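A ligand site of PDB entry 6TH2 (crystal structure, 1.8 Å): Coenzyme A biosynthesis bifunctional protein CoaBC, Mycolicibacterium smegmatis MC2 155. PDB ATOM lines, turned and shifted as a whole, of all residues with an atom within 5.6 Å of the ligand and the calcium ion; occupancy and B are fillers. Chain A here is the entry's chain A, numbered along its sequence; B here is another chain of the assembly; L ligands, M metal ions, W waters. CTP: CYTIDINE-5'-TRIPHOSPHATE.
Merely in contact with the ligand: Val 102 (3.5 Å), Ala 103 (3.7 Å), Asp 132 (3.6 Å), Gly 154 (3.6 Å) and Ala 156 (3.995 Å). Hydrophobic or aromatic side chains that line the ligand: Met 98, Val 102, Val 133, Leu 134 and Ala 156.
The side-chain carboxylate (OD2) of Asp 104 lies close to the side-chain amino group (NZ) of Lys 114 of chain B, at 3.6 Å. The backbone carbonyl oxygen of Asp 104 is in hydrogen-bond range of the backbone NH of Asn 130, 2.9 Å away. SD of Met 98 lies within hydrogen-bond range of OG1 of Thr 18 (3.3 Å). The backbone NH of Met 98 is in hydrogen-bond range of the backbone carbonyl oxygen of Val 153, at 2.8 Å. OE1 of Glu 158 lies within salt-bridge range of NZ of Lys 173, at 2.6 Å. N of Ala 100 sits at hydrogen-bond distance from O of Thr 18 (3.2 Å). The side-chain carboxylate (OD2) of Asp 132 lies within salt-bridge range of the side-chain amino group (NZ) of Lys 177, 2.9 Å away. O of Ala 103 sits at hydrogen-bond distance from ND2 of Asn 130, at 3.0 Å.
Water W4 lies within hydrogen-bond range of O3G of the ligand, OE2 of Glu 158 and NZ of Lys 116 of chain B. Water W2 lies within hydrogen-bond range of the backbone carbonyl oxygen of Ile 115 of chain B (2.8 Å) and the side-chain amino group of Lys 114 of chain B (2.8 Å). Water W1 lies within hydrogen-bond range of the side-chain carboxylate (OD2) of Asp 132 (2.9 Å), an oxygen (O1B) of the ligand (3.0 Å) and the side-chain amino group (NZ) of Lys 177 (3.2 Å).
The calcium ion is bound by O2B of the ligand, O1G of the ligand, O1A of the ligand, water W7, OD2 of Asp 104, water W5 and OD1 of Asp 104.
An oxygen (O3G) of the ligand is in salt-bridge range of the side-chain amino group (NZ) of Lys 116 of chain B (2.7 Å). The backbone NH of Leu 134 is in hydrogen-bond range of an oxygen (O2) of the ligand (2.7 Å). O3' of the ligand lies within hydrogen-bond range of O of Met 98, at 2.7 Å. The side-chain amino group (NZ) of Lys 173 lies within salt-bridge range of an oxygen (O2A) of the ligand (2.7 Å). An oxygen (O2') of the ligand sits at hydrogen-bond distance from the backbone carbonyl oxygen of Ala 100. An oxygen (O2G) of the ligand sits at hydrogen-bond distance from the backbone NH (N) of Lys 117 of chain B (2.9 Å). The backbone carbonyl oxygen of Asp 131 lies within hydrogen-bond range of a nitrogen (N4) of the ligand, 3.0 Å away. The side-chain amino group of Lys 177 lies within salt-bridge range of an oxygen (O1B) of the ligand (3.9 Å). N of Phe 155 is in hydrogen-bond range of O3' of the ligand, 3.1 Å away. An oxygen (O3') of the ligand sits close to the backbone carbonyl oxygen (O) of Phe 155 (3.4 Å). N of Val 133 sits at hydrogen-bond distance from N3 of the ligand, 3.1 Å away.
Merely in contact with the calcium ion: Lys 114 of chain B (3.9 Å). Within 4 Å of the calcium ion: Asp 104 and Lys 114 of chain B. The nearest printed residue that does not touch the calcium ion is Val 102 (4.7 Å).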
ATOM      1  N   THR A  18      37.912  -3.873   0.087  1.00  0.00           N
ATOM      2  CA  THR A  18      37.099  -3.690  -1.109  1.00  0.00           C
ATOM      3  C   THR A  18      37.238  -2.251  -1.592  1.00  0.00           C
ATOM      4  O   THR A  18      37.397  -1.336  -0.778  1.00  0.00           O
ATOM      5  CB  THR A  18      35.619  -4.053  -0.869  1.00  0.00           C
ATOM      6  OG1 THR A  18      35.008  -3.127   0.035  1.00  0.00           O
ATOM      7  CG2 THR A  18      35.480  -5.479  -0.286  1.00  0.00           C
ATOM      8  N   ALA A  79      27.309  -5.987  -6.872  1.00  0.00           N
ATOM      9  CA  ALA A  79      27.275  -6.041  -5.409  1.00  0.00           C
ATOM     10  C   ALA A  79      27.158  -7.474  -4.901  1.00  0.00           C
ATOM     11  O   ALA A  79      27.736  -7.811  -3.864  1.00  0.00           O
ATOM     12  CB  ALA A  79      26.112  -5.188  -4.879  1.00  0.00           C
ATOM     13  N   MET A  98      35.944  -1.772   4.100  1.00  0.00           N
ATOM     14  CA  MET A  98      34.888  -1.726   3.102  1.00  0.00           C
ATOM     15  C   MET A  98      34.872  -0.349   2.448  1.00  0.00           C
ATOM     16  O   MET A  98      34.064   0.527   2.785  1.00  0.00           O
ATOM     17  CB  MET A  98      33.544  -2.061   3.746  1.00  0.00           C
ATOM     18  CG  MET A  98      33.302  -3.563   3.982  1.00  0.00           C
ATOM     19  SD  MET A  98      33.371  -4.601   2.510  1.00  0.00           S
ATOM     20  CE  MET A  98      31.841  -4.162   1.705  1.00  0.00           C
ATOM     21  N   ALA A  99      35.798  -0.129   1.520  1.00  0.00           N
ATOM     22  CA  ALA A  99      35.863   1.160   0.844  1.00  0.00           C
ATOM     23  C   ALA A  99      35.093   1.164  -0.468  1.00  0.00           C
ATOM     24  O   ALA A  99      35.034   2.213  -1.130  1.00  0.00           O
ATOM     25  CB  ALA A  99      37.330   1.574   0.615  1.00  0.00           C
ATOM     26  N   ALA A 100      34.523   0.035  -0.880  1.00  0.00           N
ATOM     27  CA  ALA A 100      33.813  -0.011  -2.146  1.00  0.00           C
ATOM     28  C   ALA A 100      32.518   0.785  -2.058  1.00  0.00           C
ATOM     29  O   ALA A 100      31.900   0.884  -0.985  1.00  0.00           O
ATOM     30  CB  ALA A 100      33.527  -1.454  -2.551  1.00  0.00           C
ATOM     31  N   ALA A 101      32.134   1.399  -3.179  1.00  0.00           N
ATOM     32  CA  ALA A 101      30.807   2.013  -3.329  1.00  0.00           C
ATOM     33  C   ALA A 101      29.877   0.922  -3.845  1.00  0.00           C
ATOM     34  O   ALA A 101      29.793   0.669  -5.042  1.00  0.00           O
ATOM     35  CB  ALA A 101      30.847   3.220  -4.245  1.00  0.00           C
ATOM     36  N   VAL A 102      29.250   0.215  -2.916  1.00  0.00           N
ATOM     37  CA  VAL A 102      28.427  -0.952  -3.224  1.00  0.00           C
ATOM     38  C   VAL A 102      27.001  -0.509  -3.515  1.00  0.00           C
ATOM     39  O   VAL A 102      26.371   0.174  -2.708  1.00  0.00           O
ATOM     40  CB  VAL A 102      28.468  -1.963  -2.057  1.00  0.00           C
ATOM     41  CG1 VAL A 102      27.688  -3.243  -2.419  1.00  0.00           C
ATOM     42  CG2 VAL A 102      29.925  -2.317  -1.660  1.00  0.00           C
ATOM     43  N   ALA A 103      26.465  -0.946  -4.660  1.00  0.00           N
ATOM     44  CA  ALA A 103      25.107  -0.545  -5.040  1.00  0.00           C
ATOM     45  C   ALA A 103      24.078  -1.022  -4.021  1.00  0.00           C
ATOM     46  O   ALA A 103      24.097  -2.190  -3.629  1.00  0.00           O
ATOM     47  CB  ALA A 103      24.786  -1.132  -6.414  1.00  0.00           C
ATOM     48  N   ASP A 104      23.187  -0.113  -3.580  1.00  0.00           N
ATOM     49  CA  ASP A 104      22.114  -0.516  -2.676  1.00  0.00           C
ATOM     50  C   ASP A 104      21.059  -1.347  -3.404  1.00  0.00           C
ATOM     51  O   ASP A 104      20.397  -2.181  -2.781  1.00  0.00           O
ATOM     52  CB  ASP A 104      21.443   0.729  -2.071  1.00  0.00           C
ATOM     53  CG  ASP A 104      22.367   1.521  -1.160  1.00  0.00           C
ATOM     54  OD1 ASP A 104      23.154   0.908  -0.419  1.00  0.00           O
ATOM     55  OD2 ASP A 104      22.332   2.771  -1.230  1.00  0.00           O
ATOM     56  N   ASN A 130      20.148  -5.092  -2.716  1.00  0.00           N
ATOM     57  CA  ASN A 130      21.340  -5.925  -2.534  1.00  0.00           C
ATOM     58  C   ASN A 130      21.627  -6.078  -1.045  1.00  0.00           C
ATOM     59  O   ASN A 130      21.291  -5.228  -0.223  1.00  0.00           O
ATOM     60  CB  ASN A 130      22.546  -5.281  -3.204  1.00  0.00           C
ATOM     61  CG  ASN A 130      22.480  -5.363  -4.716  1.00  0.00           C
ATOM     62  OD1 ASN A 130      22.133  -6.395  -5.288  1.00  0.00           O
ATOM     63  ND2 ASN A 130      22.800  -4.235  -5.378  1.00  0.00           N
ATOM     64  N   ASP A 131      22.291  -7.176  -0.690  1.00  0.00           N
ATOM     65  CA  ASP A 131      22.664  -7.372   0.703  1.00  0.00           C
ATOM     66  C   ASP A 131      23.669  -6.326   1.149  1.00  0.00           C
ATOM     67  O   ASP A 131      24.563  -5.922   0.388  1.00  0.00           O
ATOM     68  CB  ASP A 131      23.251  -8.774   0.913  1.00  0.00           C
ATOM     69  CG  ASP A 131      22.226  -9.876   0.732  1.00  0.00           C
ATOM     70  OD1 ASP A 131      21.015  -9.561   0.629  1.00  0.00           O
ATOM     71  OD2 ASP A 131      22.631 -11.050   0.707  1.00  0.00           O
ATOM     72  N   ASP A 132      23.528  -5.890   2.397  1.00  0.00           N
ATOM     73  CA  ASP A 132      24.485  -5.004   3.064  1.00  0.00           C
ATOM     74  C   ASP A 132      25.666  -5.844   3.524  1.00  0.00           C
ATOM     75  O   ASP A 132      25.576  -6.587   4.515  1.00  0.00           O
ATOM     76  CB  ASP A 132      23.799  -4.320   4.245  1.00  0.00           C
ATOM     77  CG  ASP A 132      24.639  -3.225   4.855  1.00  0.00           C
ATOM     78  OD1 ASP A 132      25.880  -3.304   4.830  1.00  0.00           O
ATOM     79  OD2 ASP A 132      24.043  -2.310   5.445  1.00  0.00           O
ATOM     80  N   VAL A 133      26.783  -5.751   2.806  1.00  0.00           N
ATOM     81  CA  VAL A 133      27.923  -6.635   3.081  1.00  0.00           C
ATOM     82  C   VAL A 133      28.611  -6.225   4.376  1.00  0.00           C
ATOM     83  O   VAL A 133      28.955  -7.076   5.203  1.00  0.00           O
ATOM     84  CB  VAL A 133      28.902  -6.625   1.887  1.00  0.00           C
ATOM     85  CG1 VAL A 133      30.092  -7.536   2.182  1.00  0.00           C
ATOM     86  CG2 VAL A 133      28.193  -7.055   0.621  1.00  0.00           C
ATOM     87  N   LEU A 134      28.816  -4.920   4.571  1.00  0.00           N
ATOM     88  CA  LEU A 134      29.408  -4.425   5.807  1.00  0.00           C
ATOM     89  C   LEU A 134      28.608  -4.861   7.039  1.00  0.00           C
ATOM     90  O   LEU A 134      29.170  -5.353   8.022  1.00  0.00           O
ATOM     91  CB  LEU A 134      29.500  -2.898   5.748  1.00  0.00           C
ATOM     92  CG  LEU A 134      29.912  -2.184   7.032  1.00  0.00           C
ATOM     93  CD1 LEU A 134      31.333  -2.583   7.429  1.00  0.00           C
ATOM     94  CD2 LEU A 134      29.826  -0.680   6.871  1.00  0.00           C
ATOM     95  N   ALA A 135      27.286  -4.648   7.005  1.00  0.00           N
ATOM     96  CA  ALA A 135      26.452  -5.063   8.133  1.00  0.00           C
ATOM     97  C   ALA A 135      26.497  -6.564   8.323  1.00  0.00           C
ATOM     98  O   ALA A 135      26.497  -7.054   9.469  1.00  0.00           O
ATOM     99  CB  ALA A 135      25.018  -4.584   7.915  1.00  0.00           C
ATOM    100  N   VAL A 153      36.049  -1.922   9.155  1.00  0.00           N
ATOM    101  CA  VAL A 153      36.102  -0.494   8.828  1.00  0.00           C
ATOM    102  C   VAL A 153      35.106  -0.216   7.721  1.00  0.00           C
ATOM    103  O   VAL A 153      35.193  -0.808   6.632  1.00  0.00           O
ATOM    104  CB  VAL A 153      37.511  -0.067   8.363  1.00  0.00           C
ATOM    105  CG1 VAL A 153      37.530   1.433   8.069  1.00  0.00           C
ATOM    106  CG2 VAL A 153      38.571  -0.448   9.386  1.00  0.00           C
ATOM    107  N   GLY A 154      34.184   0.720   7.961  1.00  0.00           N
ATOM    108  CA  GLY A 154      33.296   1.183   6.917  1.00  0.00           C
ATOM    109  C   GLY A 154      33.705   2.563   6.410  1.00  0.00           C
ATOM    110  O   GLY A 154      34.486   3.280   7.034  1.00  0.00           O
ATOM    111  N   PHE A 155      33.175   2.904   5.232  1.00  0.00           N
ATOM    112  CA  PHE A 155      33.365   4.196   4.590  1.00  0.00           C
ATOM    113  C   PHE A 155      31.998   4.803   4.325  1.00  0.00           C
ATOM    114  O   PHE A 155      31.035   4.082   4.063  1.00  0.00           O
ATOM    115  CB  PHE A 155      34.128   4.069   3.255  1.00  0.00           C
ATOM    116  CG  PHE A 155      35.609   4.002   3.402  1.00  0.00           C
ATOM    117  CD1 PHE A 155      36.203   2.942   4.064  1.00  0.00           C
ATOM    118  CD2 PHE A 155      36.398   5.015   2.909  1.00  0.00           C
ATOM    119  CE1 PHE A 155      37.578   2.887   4.215  1.00  0.00           C
ATOM    120  CE2 PHE A 155      37.769   4.961   3.050  1.00  0.00           C
ATOM    121  CZ  PHE A 155      38.358   3.892   3.703  1.00  0.00           C
ATOM    122  N   ALA A 156      31.901   6.130   4.400  1.00  0.00           N
ATOM    123  CA  ALA A 156      30.631   6.778   4.099  1.00  0.00           C
ATOM    124  C   ALA A 156      30.895   8.151   3.488  1.00  0.00           C
ATOM    125  O   ALA A 156      31.843   8.835   3.874  1.00  0.00           O
ATOM    126  CB  ALA A 156      29.761   6.914   5.339  1.00  0.00           C
ATOM    127  N   ALA A 157      30.074   8.521   2.515  1.00  0.00           N
ATOM    128  CA  ALA A 157      30.008   9.884   2.001  1.00  0.00           C
ATOM    129  C   ALA A 157      28.739  10.505   2.560  1.00  0.00           C
ATOM    130  O   ALA A 157      27.627  10.036   2.259  1.00  0.00           O
ATOM    131  CB  ALA A 157      29.998   9.887   0.475  1.00  0.00           C
ATOM    132  N   GLU A 158      28.885  11.543   3.372  1.00  0.00           N
ATOM    133  CA  GLU A 158      27.741  12.154   4.018  1.00  0.00           C
ATOM    134  C   GLU A 158      27.698  13.644   3.684  1.00  0.00           C
ATOM    135  O   GLU A 158      28.732  14.270   3.425  1.00  0.00           O
ATOM    136  CB  GLU A 158      27.787  12.005   5.556  1.00  0.00           C
ATOM    137  CG  GLU A 158      27.807  10.572   6.126  1.00  0.00           C
ATOM    138  CD  GLU A 158      26.571   9.757   5.783  1.00  0.00           C
ATOM    139  OE1 GLU A 158      26.684   8.516   5.755  1.00  0.00           O
ATOM    140  OE2 GLU A 158      25.477  10.325   5.626  1.00  0.00           O
ATOM    141  N   LYS A 173      25.159   6.933  11.012  1.00  0.00           N
ATOM    142  CA  LYS A 173      25.595   5.841  10.164  1.00  0.00           C
ATOM    143  C   LYS A 173      26.539   4.926  10.924  1.00  0.00           C
ATOM    144  O   LYS A 173      26.390   3.706  10.868  1.00  0.00           O
ATOM    145  CB  LYS A 173      26.260   6.416   8.897  1.00  0.00           C
ATOM    146  CG  LYS A 173      26.682   5.420   7.847  1.00  0.00           C
ATOM    147  CD  LYS A 173      25.511   4.696   7.236  1.00  0.00           C
ATOM    148  CE  LYS A 173      24.559   5.621   6.481  1.00  0.00           C
ATOM    149  NZ  LYS A 173      25.261   6.400   5.407  1.00  0.00           N
ATOM    150  N   LYS A 177      25.531   0.989  11.478  1.00  0.00           N
ATOM    151  CA  LYS A 177      26.368  -0.056  10.913  1.00  0.00           C
ATOM    152  C   LYS A 177      27.020  -0.899  11.991  1.00  0.00           C
ATOM    153  O   LYS A 177      27.185  -2.115  11.802  1.00  0.00           O
ATOM    154  CB  LYS A 177      27.431   0.561   9.995  1.00  0.00           C
ATOM    155  CG  LYS A 177      26.867   1.224   8.727  1.00  0.00           C
ATOM    156  CD  LYS A 177      26.390   0.197   7.707  1.00  0.00           C
ATOM    157  CE  LYS A 177      26.146   0.793   6.306  1.00  0.00           C
ATOM    158  NZ  LYS A 177      26.057  -0.272   5.204  1.00  0.00           N
ATOM    159  N   LYS B 114      21.732  11.816  -3.788  1.00  0.00           N
ATOM    160  CA  LYS B 114      21.780  10.369  -3.954  1.00  0.00           C
ATOM    161  C   LYS B 114      20.586   9.723  -3.279  1.00  0.00           C
ATOM    162  O   LYS B 114      20.263  10.025  -2.122  1.00  0.00           O
ATOM    163  CB  LYS B 114      23.076   9.801  -3.381  1.00  0.00           C
ATOM    164  CG  LYS B 114      23.365   8.366  -3.824  1.00  0.00           C
ATOM    165  CD  LYS B 114      24.689   7.866  -3.277  1.00  0.00           C
ATOM    166  CE  LYS B 114      24.921   6.389  -3.590  1.00  0.00           C
ATOM    167  NZ  LYS B 114      23.944   5.475  -2.918  1.00  0.00           N
ATOM    168  N   ILE B 115      19.894   8.863  -4.023  1.00  0.00           N
ATOM    169  CA  ILE B 115      18.725   8.172  -3.484  1.00  0.00           C
ATOM    170  C   ILE B 115      19.139   7.348  -2.279  1.00  0.00           C
ATOM    171  O   ILE B 115      20.091   6.568  -2.328  1.00  0.00           O
ATOM    172  CB  ILE B 115      18.072   7.300  -4.563  1.00  0.00           C
ATOM    173  CG1 ILE B 115      17.433   8.181  -5.643  1.00  0.00           C
ATOM    174  CG2 ILE B 115      17.018   6.389  -3.945  1.00  0.00           C
ATOM    175  CD1 ILE B 115      18.060   8.039  -6.987  1.00  0.00           C
ATOM    176  N   LYS B 116      18.421   7.527  -1.175  1.00  0.00           N
ATOM    177  CA  LYS B 116      18.742   6.871   0.088  1.00  0.00           C
ATOM    178  C   LYS B 116      18.104   5.496   0.168  1.00  0.00           C
ATOM    179  O   LYS B 116      17.012   5.251  -0.356  1.00  0.00           O
ATOM    180  CB  LYS B 116      18.266   7.723   1.264  1.00  0.00           C
ATOM    181  CG  LYS B 116      19.311   8.667   1.824  1.00  0.00           C
ATOM    182  CD  LYS B 116      19.074   8.886   3.317  1.00  0.00           C
ATOM    183  CE  LYS B 116      20.328   9.403   4.011  1.00  0.00           C
ATOM    184  NZ  LYS B 116      21.394   8.360   4.070  1.00  0.00           N
ATOM    185  N   LYS B 117      18.806   4.585   0.824  1.00  0.00           N
ATOM    186  CA  LYS B 117      18.318   3.230   1.094  1.00  0.00           C
ATOM    187  C   LYS B 117      17.280   3.334   2.206  1.00  0.00           C
ATOM    188  O   LYS B 117      17.621   3.468   3.388  1.00  0.00           O
ATOM    189  CB  LYS B 117      19.473   2.327   1.481  1.00  0.00           C
ATOM    190  CG  LYS B 117      19.157   0.846   1.543  1.00  0.00           C
ATOM    191  CD  LYS B 117      20.294   0.085   2.238  1.00  0.00           C
ATOM    192  N   GLY B 118      16.001   3.301   1.840  1.00  0.00           N
ATOM    193  CA  GLY B 118      14.971   3.390   2.848  1.00  0.00           C
ATOM    194  C   GLY B 118      14.718   2.062   3.524  1.00  0.00           C
ATOM    195  O   GLY B 118      15.647   1.268   3.725  1.00  0.00           O
HETATM  196  N1  CTP L   1      28.122  -1.217   1.818  1.00  0.00           N
HETATM  197  C2  CTP L   1      27.971  -2.591   1.811  1.00  0.00           C
HETATM  198  N3  CTP L   1      26.937  -3.175   1.135  1.00  0.00           N
HETATM  199  C4  CTP L   1      25.958  -2.399   0.549  1.00  0.00           C
HETATM  200  C5  CTP L   1      26.037  -1.014   0.665  1.00  0.00           C
HETATM  201  C6  CTP L   1      27.109  -0.423   1.326  1.00  0.00           C
HETATM  202  O2  CTP L   1      28.789  -3.299   2.419  1.00  0.00           O
HETATM  203  N4  CTP L   1      24.951  -2.978  -0.093  1.00  0.00           N
HETATM  204  C1' CTP L   1      29.158  -0.613   2.648  1.00  0.00           C
HETATM  205  C2' CTP L   1      30.124   0.269   1.857  1.00  0.00           C
HETATM  206  O2' CTP L   1      31.234  -0.449   1.355  1.00  0.00           O
HETATM  207  C3' CTP L   1      30.555   1.291   2.873  1.00  0.00           C
HETATM  208  C4' CTP L   1      29.307   1.446   3.720  1.00  0.00           C
HETATM  209  O4' CTP L   1      28.551   0.249   3.598  1.00  0.00           O
HETATM  210  O3' CTP L   1      31.550   0.787   3.746  1.00  0.00           O
HETATM  211  C5' CTP L   1      28.507   2.596   3.122  1.00  0.00           C
HETATM  212  O5' CTP L   1      27.179   2.495   3.557  1.00  0.00           O
HETATM  213  PA  CTP L   1      26.147   3.668   3.149  1.00  0.00           P
HETATM  214  O1A CTP L   1      25.913   3.623   1.670  1.00  0.00           O
HETATM  215  O2A CTP L   1      26.733   4.984   3.587  1.00  0.00           O
HETATM  216  O3A CTP L   1      24.944   3.247   4.085  1.00  0.00           O
HETATM  217  PB  CTP L   1      23.487   2.870   3.602  1.00  0.00           P
HETATM  218  O1B CTP L   1      22.874   1.942   4.632  1.00  0.00           O
HETATM  219  O2B CTP L   1      23.455   2.281   2.214  1.00  0.00           O
HETATM  220  O3B CTP L   1      22.784   4.300   3.773  1.00  0.00           O
HETATM  221  PG  CTP L   1      22.498   5.339   2.593  1.00  0.00           P
HETATM  222  O1G CTP L   1      23.097   4.864   1.299  1.00  0.00           O
HETATM  223  O2G CTP L   1      20.997   5.549   2.449  1.00  0.00           O
HETATM  224  O3G CTP L   1      23.150   6.651   2.981  1.00  0.00           O
HETATM  225 CA    CA M   1      24.156   3.102   0.227  1.00  0.00          CA
HETATM  226  O   HOH W   1      23.567  -0.619   3.154  1.00  0.00           O
HETATM  227  O   HOH W   2      22.392   6.506  -0.780  1.00  0.00           O
HETATM  228  O   HOH W   3      22.731  -1.406   0.511  1.00  0.00           O
HETATM  229  O   HOH W   4      24.209   9.108   3.206  1.00  0.00           O
HETATM  230  O   HOH W   5      25.222   4.976  -0.799  1.00  0.00           O
HETATM  231  O   HOH W   6      25.257   6.767   1.318  1.00  0.00           O
HETATM  232  O   HOH W   7      25.864   2.020  -0.966  1.00  0.00           O
